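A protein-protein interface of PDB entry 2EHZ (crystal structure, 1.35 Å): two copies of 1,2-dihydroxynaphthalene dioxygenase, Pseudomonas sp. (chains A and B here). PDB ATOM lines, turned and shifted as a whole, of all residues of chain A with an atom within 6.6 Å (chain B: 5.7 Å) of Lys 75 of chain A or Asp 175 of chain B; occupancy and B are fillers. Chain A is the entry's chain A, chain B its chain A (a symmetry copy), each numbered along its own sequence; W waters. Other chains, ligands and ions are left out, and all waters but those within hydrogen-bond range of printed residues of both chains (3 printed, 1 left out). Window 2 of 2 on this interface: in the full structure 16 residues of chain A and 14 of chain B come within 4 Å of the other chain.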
ATOM      1  N   VAL A  72     -16.133  20.694   9.205  1.00  0.00           N
ATOM      2  CA  VAL A  72     -17.551  20.508   9.522  1.00  0.00           C
ATOM      3  C   VAL A  72     -18.122  19.462   8.560  1.00  0.00           C
ATOM      4  O   VAL A  72     -17.493  19.132   7.543  1.00  0.00           O
ATOM      5  CB  VAL A  72     -18.359  21.832   9.468  1.00  0.00           C
ATOM      6  CG1 VAL A  72     -17.806  22.842  10.470  1.00  0.00           C
ATOM      7  CG2 VAL A  72     -18.367  22.415   8.062  1.00  0.00           C
ATOM      8  N   ALA A  73     -19.299  18.935   8.879  1.00  0.00           N
ATOM      9  CA  ALA A  73     -19.825  17.787   8.141  1.00  0.00           C
ATOM     10  C   ALA A  73     -20.100  18.084   6.671  1.00  0.00           C
ATOM     11  O   ALA A  73     -19.782  17.267   5.805  1.00  0.00           O
ATOM     12  CB  ALA A  73     -21.065  17.216   8.830  1.00  0.00           C
ATOM     13  N   GLY A  74     -20.666  19.248   6.381  1.00  0.00           N
ATOM     14  CA  GLY A  74     -21.003  19.596   5.007  1.00  0.00           C
ATOM     15  C   GLY A  74     -21.324  21.064   4.855  1.00  0.00           C
ATOM     16  O   GLY A  74     -21.152  21.858   5.790  1.00  0.00           O
ATOM     17  N   LYS A  75     -21.798  21.425   3.666  1.00  0.00           N
ATOM     18  CA  LYS A  75     -22.116  22.803   3.345  1.00  0.00           C
ATOM     19  C   LYS A  75     -23.149  23.446   4.290  1.00  0.00           C
ATOM     20  O   LYS A  75     -22.974  24.608   4.670  1.00  0.00           O
ATOM     21  CB  LYS A  75     -22.550  22.930   1.877  1.00  0.00           C
ATOM     22  CG  LYS A  75     -22.511  24.356   1.351  1.00  0.00           C
ATOM     23  CD  LYS A  75     -23.121  24.494  -0.048  1.00  0.00           C
ATOM     24  CE  LYS A  75     -22.124  24.147  -1.143  1.00  0.00           C
ATOM     25  NZ  LYS A  75     -22.640  24.520  -2.497  1.00  0.00           N
ATOM     26  N   PRO A  76     -24.230  22.713   4.663  1.00  0.00           N
ATOM     27  CA  PRO A  76     -25.197  23.363   5.566  1.00  0.00           C
ATOM     28  C   PRO A  76     -24.595  23.778   6.909  1.00  0.00           C
ATOM     29  O   PRO A  76     -24.911  24.853   7.419  1.00  0.00           O
ATOM     30  CB  PRO A  76     -26.280  22.290   5.764  1.00  0.00           C
ATOM     31  CG  PRO A  76     -26.155  21.387   4.575  1.00  0.00           C
ATOM     32  CD  PRO A  76     -24.675  21.353   4.290  1.00  0.00           C
ATOM     33  N   GLU A  77     -23.721  22.942   7.462  1.00  0.00           N
ATOM     34  CA  GLU A  77     -23.071  23.238   8.740  1.00  0.00           C
ATOM     35  C   GLU A  77     -22.027  24.348   8.589  1.00  0.00           C
ATOM     36  O   GLU A  77     -21.875  25.187   9.481  1.00  0.00           O
ATOM     37  CB  GLU A  77     -22.433  21.969   9.312  1.00  0.00           C
ATOM     38  CG  GLU A  77     -23.435  20.868   9.698  1.00  0.00           C
ATOM     39  CD  GLU A  77     -23.985  20.077   8.509  1.00  0.00           C
ATOM     40  OE1 GLU A  77     -23.323  20.009   7.454  1.00  0.00           O
ATOM     41  OE2 GLU A  77     -25.094  19.514   8.634  1.00  0.00           O
ATOM     42  N   PHE A  78     -21.332  24.356   7.450  1.00  0.00           N
ATOM     43  CA  PHE A  78     -20.385  25.416   7.079  1.00  0.00           C
ATOM     44  C   PHE A  78     -21.094  26.771   7.077  1.00  0.00           C
ATOM     45  O   PHE A  78     -20.641  27.720   7.711  1.00  0.00           O
ATOM     46  CB  PHE A  78     -19.806  25.081   5.699  1.00  0.00           C
ATOM     47  CG  PHE A  78     -18.826  26.088   5.157  1.00  0.00           C
ATOM     48  CD1 PHE A  78     -17.481  26.044   5.522  1.00  0.00           C
ATOM     49  CD2 PHE A  78     -19.231  27.038   4.225  1.00  0.00           C
ATOM     50  CE1 PHE A  78     -16.567  26.956   4.994  1.00  0.00           C
ATOM     51  CE2 PHE A  78     -18.323  27.954   3.692  1.00  0.00           C
ATOM     52  CZ  PHE A  78     -16.991  27.913   4.079  1.00  0.00           C
ATOM     53  N   GLU A  79     -22.221  26.844   6.379  1.00  0.00           N
ATOM     54  CA  GLU A  79     -22.972  28.089   6.271  1.00  0.00           C
ATOM     55  C   GLU A  79     -23.548  28.526   7.612  1.00  0.00           C
ATOM     56  O   GLU A  79     -23.494  29.712   7.959  1.00  0.00           O
ATOM     57  CB  GLU A  79     -24.067  27.950   5.210  1.00  0.00           C
ATOM     58  CG  GLU A  79     -23.500  27.829   3.803  1.00  0.00           C
ATOM     59  CD  GLU A  79     -24.558  27.733   2.719  1.00  0.00           C
ATOM     60  OE1 GLU A  79     -24.172  27.703   1.531  1.00  0.00           O
ATOM     61  OE2 GLU A  79     -25.761  27.673   3.047  1.00  0.00           O
ATOM     62  N   ALA A  80     -24.082  27.572   8.371  1.00  0.00           N
ATOM     63  CA  ALA A  80     -24.656  27.867   9.683  1.00  0.00           C
ATOM     64  C   ALA A  80     -23.606  28.396  10.657  1.00  0.00           C
ATOM     65  O   ALA A  80     -23.850  29.370  11.372  1.00  0.00           O
ATOM     66  CB  ALA A  80     -25.364  26.647  10.251  1.00  0.00           C
ATOM     67  N   LEU A 106     -13.651  21.596  -0.466  1.00  0.00           N
ATOM     68  CA  LEU A 106     -14.783  22.091  -1.267  1.00  0.00           C
ATOM     69  C   LEU A 106     -15.299  23.461  -0.843  1.00  0.00           C
ATOM     70  O   LEU A 106     -15.808  24.212  -1.673  1.00  0.00           O
ATOM     71  CB  LEU A 106     -15.919  21.071  -1.318  1.00  0.00           C
ATOM     72  CG  LEU A 106     -15.534  19.744  -1.979  1.00  0.00           C
ATOM     73  CD1 LEU A 106     -16.688  18.776  -1.888  1.00  0.00           C
ATOM     74  CD2 LEU A 106     -15.080  19.919  -3.429  1.00  0.00           C
ATOM     75  N   TRP A 123     -15.353  22.367   4.678  1.00  0.00           N
ATOM     76  CA  TRP A 123     -16.026  21.099   4.441  1.00  0.00           C
ATOM     77  C   TRP A 123     -15.462  20.452   3.184  1.00  0.00           C
ATOM     78  O   TRP A 123     -14.963  21.140   2.289  1.00  0.00           O
ATOM     79  CB  TRP A 123     -17.553  21.266   4.343  1.00  0.00           C
ATOM     80  CG  TRP A 123     -18.046  21.928   3.084  1.00  0.00           C
ATOM     81  CD1 TRP A 123     -18.168  23.268   2.850  1.00  0.00           C
ATOM     82  CD2 TRP A 123     -18.504  21.269   1.900  1.00  0.00           C
ATOM     83  NE1 TRP A 123     -18.667  23.485   1.586  1.00  0.00           N
ATOM     84  CE2 TRP A 123     -18.881  22.274   0.980  1.00  0.00           C
ATOM     85  CE3 TRP A 123     -18.627  19.929   1.524  1.00  0.00           C
ATOM     86  CZ2 TRP A 123     -19.370  21.980  -0.299  1.00  0.00           C
ATOM     87  CZ3 TRP A 123     -19.125  19.634   0.250  1.00  0.00           C
ATOM     88  CH2 TRP A 123     -19.486  20.660  -0.644  1.00  0.00           C
ATOM     89  N   HIS B 164     -30.030  19.746  -6.354  1.00  0.00           N
ATOM     90  CA  HIS B 164     -29.647  19.588  -4.955  1.00  0.00           C
ATOM     91  C   HIS B 164     -30.694  20.184  -4.002  1.00  0.00           C
ATOM     92  O   HIS B 164     -31.036  19.580  -2.987  1.00  0.00           O
ATOM     93  CB  HIS B 164     -28.270  20.197  -4.706  1.00  0.00           C
ATOM     94  CG  HIS B 164     -27.759  19.943  -3.328  1.00  0.00           C
ATOM     95  ND1 HIS B 164     -28.116  20.719  -2.247  1.00  0.00           N
ATOM     96  CD2 HIS B 164     -26.953  18.969  -2.844  1.00  0.00           C
ATOM     97  CE1 HIS B 164     -27.529  20.251  -1.159  1.00  0.00           C
ATOM     98  NE2 HIS B 164     -26.817  19.190  -1.496  1.00  0.00           N
ATOM     99  N   ARG B 173     -29.290  13.903   1.704  1.00  0.00           N
ATOM    100  CA  ARG B 173     -28.062  14.583   2.089  1.00  0.00           C
ATOM    101  C   ARG B 173     -26.954  14.183   1.127  1.00  0.00           C
ATOM    102  O   ARG B 173     -26.897  13.036   0.687  1.00  0.00           O
ATOM    103  CB  ARG B 173     -27.700  14.155   3.517  1.00  0.00           C
ATOM    104  CG  ARG B 173     -26.304  14.514   3.982  1.00  0.00           C
ATOM    105  CD  ARG B 173     -26.345  15.484   5.120  1.00  0.00           C
ATOM    106  NE  ARG B 173     -25.001  15.896   5.506  1.00  0.00           N
ATOM    107  CZ  ARG B 173     -24.725  17.037   6.128  1.00  0.00           C
ATOM    108  NH1 ARG B 173     -25.701  17.886   6.430  1.00  0.00           N
ATOM    109  NH2 ARG B 173     -23.472  17.332   6.437  1.00  0.00           N
ATOM    110  N   GLY B 174     -26.069  15.117   0.808  1.00  0.00           N
ATOM    111  CA  GLY B 174     -24.920  14.815  -0.042  1.00  0.00           C
ATOM    112  C   GLY B 174     -24.564  15.971  -0.942  1.00  0.00           C
ATOM    113  O   GLY B 174     -25.344  16.904  -1.099  1.00  0.00           O
ATOM    114  N   ASP B 175     -23.387  15.902  -1.546  1.00  0.00           N
ATOM    115  CA  ASP B 175     -22.905  16.996  -2.383  1.00  0.00           C
ATOM    116  C   ASP B 175     -21.913  16.437  -3.401  1.00  0.00           C
ATOM    117  O   ASP B 175     -21.913  15.223  -3.674  1.00  0.00           O
ATOM    118  CB  ASP B 175     -22.290  18.107  -1.506  1.00  0.00           C
ATOM    119  CG  ASP B 175     -22.551  19.500  -2.057  1.00  0.00           C
ATOM    120  OD1 ASP B 175     -22.110  19.778  -3.182  1.00  0.00           O
ATOM    121  OD2 ASP B 175     -23.193  20.322  -1.361  1.00  0.00           O
ATOM    122  N   VAL B 176     -21.081  17.305  -3.965  1.00  0.00           N
ATOM    123  CA  VAL B 176     -20.041  16.887  -4.896  1.00  0.00           C
ATOM    124  C   VAL B 176     -19.089  15.919  -4.194  1.00  0.00           C
ATOM    125  O   VAL B 176     -18.490  16.267  -3.172  1.00  0.00           O
ATOM    126  CB  VAL B 176     -19.252  18.103  -5.420  1.00  0.00           C
ATOM    127  CG1 VAL B 176     -18.055  17.655  -6.252  1.00  0.00           C
ATOM    128  CG2 VAL B 176     -20.169  19.015  -6.243  1.00  0.00           C
ATOM    129  N   GLU B 177     -18.962  14.704  -4.733  1.00  0.00           N
ATOM    130  CA  GLU B 177     -18.021  13.716  -4.184  1.00  0.00           C
ATOM    131  C   GLU B 177     -16.898  13.378  -5.150  1.00  0.00           C
ATOM    132  O   GLU B 177     -15.906  12.782  -4.746  1.00  0.00           O
ATOM    133  CB  GLU B 177     -18.730  12.433  -3.713  1.00  0.00           C
ATOM    134  CG  GLU B 177     -19.595  12.658  -2.483  1.00  0.00           C
ATOM    135  CD  GLU B 177     -20.351  11.431  -2.017  1.00  0.00           C
ATOM    136  OE1 GLU B 177     -20.282  10.373  -2.683  1.00  0.00           O
ATOM    137  OE2 GLU B 177     -21.033  11.535  -0.972  1.00  0.00           O
ATOM    138  N   LEU B 190     -19.431  15.417  -9.925  1.00  0.00           N
ATOM    139  CA  LEU B 190     -20.564  14.521  -9.711  1.00  0.00           C
ATOM    140  C   LEU B 190     -21.005  14.570  -8.263  1.00  0.00           C
ATOM    141  O   LEU B 190     -20.169  14.487  -7.354  1.00  0.00           O
ATOM    142  CB  LEU B 190     -20.213  13.086 -10.104  1.00  0.00           C
ATOM    143  CG  LEU B 190     -19.836  12.845 -11.568  1.00  0.00           C
ATOM    144  CD1 LEU B 190     -19.554  11.369 -11.793  1.00  0.00           C
ATOM    145  CD2 LEU B 190     -20.921  13.335 -12.530  1.00  0.00           C
ATOM    146  N   SER B 191     -22.312  14.718  -8.065  1.00  0.00           N
ATOM    147  CA  SER B 191     -22.925  14.814  -6.739  1.00  0.00           C
ATOM    148  C   SER B 191     -23.713  13.553  -6.415  1.00  0.00           C
ATOM    149  O   SER B 191     -24.356  12.980  -7.295  1.00  0.00           O
ATOM    150  CB  SER B 191     -23.851  16.027  -6.666  1.00  0.00           C
ATOM    151  OG  SER B 191     -23.114  17.215  -6.874  1.00  0.00           O
ATOM    152  N   PHE B 192     -23.666  13.138  -5.151  1.00  0.00           N
ATOM    153  CA  PHE B 192     -24.248  11.862  -4.714  1.00  0.00           C
ATOM    154  C   PHE B 192     -25.024  12.090  -3.440  1.00  0.00           C
ATOM    155  O   PHE B 192     -24.483  12.658  -2.487  1.00  0.00           O
ATOM    156  CB  PHE B 192     -23.145  10.825  -4.443  1.00  0.00           C
ATOM    157  CG  PHE B 192     -22.365  10.441  -5.668  1.00  0.00           C
ATOM    158  CD1 PHE B 192     -21.378  11.279  -6.171  1.00  0.00           C
ATOM    159  CD2 PHE B 192     -22.636   9.252  -6.337  1.00  0.00           C
ATOM    160  CE1 PHE B 192     -20.671  10.938  -7.325  1.00  0.00           C
ATOM    161  CE2 PHE B 192     -21.926   8.906  -7.489  1.00  0.00           C
ATOM    162  CZ  PHE B 192     -20.949   9.750  -7.979  1.00  0.00           C
ATOM    163  N   MET B 193     -26.280  11.644  -3.415  1.00  0.00           N
ATOM    164  CA  MET B 193     -27.140  11.904  -2.274  1.00  0.00           C
ATOM    165  C   MET B 193     -27.760  10.637  -1.707  1.00  0.00           C
ATOM    166  O   MET B 193     -28.154   9.725  -2.442  1.00  0.00           O
ATOM    167  CB  MET B 193     -28.208  12.942  -2.634  1.00  0.00           C
ATOM    168  CG  MET B 193     -27.601  14.254  -3.143  1.00  0.00           C
ATOM    169  SD  MET B 193     -28.794  15.584  -3.361  1.00  0.00           S
ATOM    170  CE  MET B 193     -28.959  16.160  -1.678  1.00  0.00           C
ATOM    171  N   ALA B 278     -19.246  14.977   4.381  1.00  0.00           N
ATOM    172  CA  ALA B 278     -18.882  15.138   2.981  1.00  0.00           C
ATOM    173  C   ALA B 278     -17.379  15.005   2.766  1.00  0.00           C
ATOM    174  O   ALA B 278     -16.583  15.666   3.444  1.00  0.00           O
ATOM    175  CB  ALA B 278     -19.357  16.501   2.480  1.00  0.00           C
HETATM  176  O   HOH W   1     -22.160  19.447   1.753  1.00  0.00           O
HETATM  177  O   HOH W   2     -21.419  22.240  -3.966  1.00  0.00           O
HETATM  178  O   HOH W   3     -24.793  22.400  -2.606  1.00  0.00           O
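The backbone carbonyl oxygen (O) of Ala 73 of chain A lies within hydrogen-bond range of the backbone NH (N) of Ala 278 of chain B (2.7 Å).
The side-chain carboxylate (OE2) of Glu 77 of chain A lies within salt-bridge range of the guanidinium group (NH1) of Arg 173 of chain B, 2.8 Å away.
The guanidinium group (NH2) of Arg 173 of chain B sits close to the backbone NH (N) of Gly 74 of chain A (3.4 Å).
OE1 of Glu 77 of chain A sits at hydrogen-bond distance from N of Gly 74 of chain A.
The backbone NH of Leu 106 of chain A is in hydrogen-bond range of the backbone carbonyl oxygen of Trp 123 of chain A (3.1 Å).
The backbone carbonyl oxygen (O) of Asp 175 of chain B lies within hydrogen-bond range of the backbone NH (N) of Phe 192 of chain B (3.1 Å).
NH2 of Arg 173 of chain B touches CB of Ala 73 of chain A, at 3.4 Å.
OD2 of Asp 175 of chain B touches CE of Lys 75 of chain A, at 3.98 Å.
Arg 173 of chain B touches Pro 76 of chain A.
Leu 106 of chain A touches Val 176 of chain B (CD1 to O, 3.3 Å).
CG of Asp 175 of chain B touches CH2 of Trp 123 of chain A, at 3.6 Å.
Trp 123 of chain A touches Ala 278 of chain B (CE3 to CB, 3.6 Å).
Printed residues of chain B within 4 Å of Ala 73 of chain A: Arg 173 and Ala 278.
Lys 75 of chain A touches just one residue of chain B: Asp 175 (3.98 Å).
Printed residues of chain B within 4 Å of Glu 77 of chain A: Arg 173 (2.8 Å).
Of the printed residues of chain A, Arg 173 of chain B touches Ala 73, Gly 74, Pro 76 and Glu 77.
The nearest residue of chain B that does not touch Lys 75 of chain A is Arg 173 of chain B (5.2 Å).
The nearest residue of chain A that does not touch Asp 175 of chain B is Leu 106 of chain A (5.7 Å).
The nearest printed residue of chain B that does not touch Trp 123 of chain A is Val 176 of chain B (4.8 Å).
Of the 11 printed residues of chain A, 7 touch a printed residue of chain B.
Printed residues of chain A that touch a printed residue of chain B: Ala 73, Gly 74, Lys 75, Pro 76, Glu 77, Leu 106 and Trp 123.
Among the printed residues, 9 pairs touch across the chains.
No position is printed for both chains.
Of the 9 pairs that touch across the chains among the printed residues, none has its exchanged pair printed and touching as well.
Water W2 bridges the side-chain carboxylate of Asp 175 of chain B and the side-chain amino group of Lys 75 of chain A.
Water W1 lies within hydrogen-bond range of the backbone NH of Lys 75 of chain A and the side-chain carboxylate of Asp 175 of chain B.
Water W3 bridges OD2 of Asp 175 of chain B (2.9 Å) and NZ of Lys 75 of chain A (3.0 Å).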
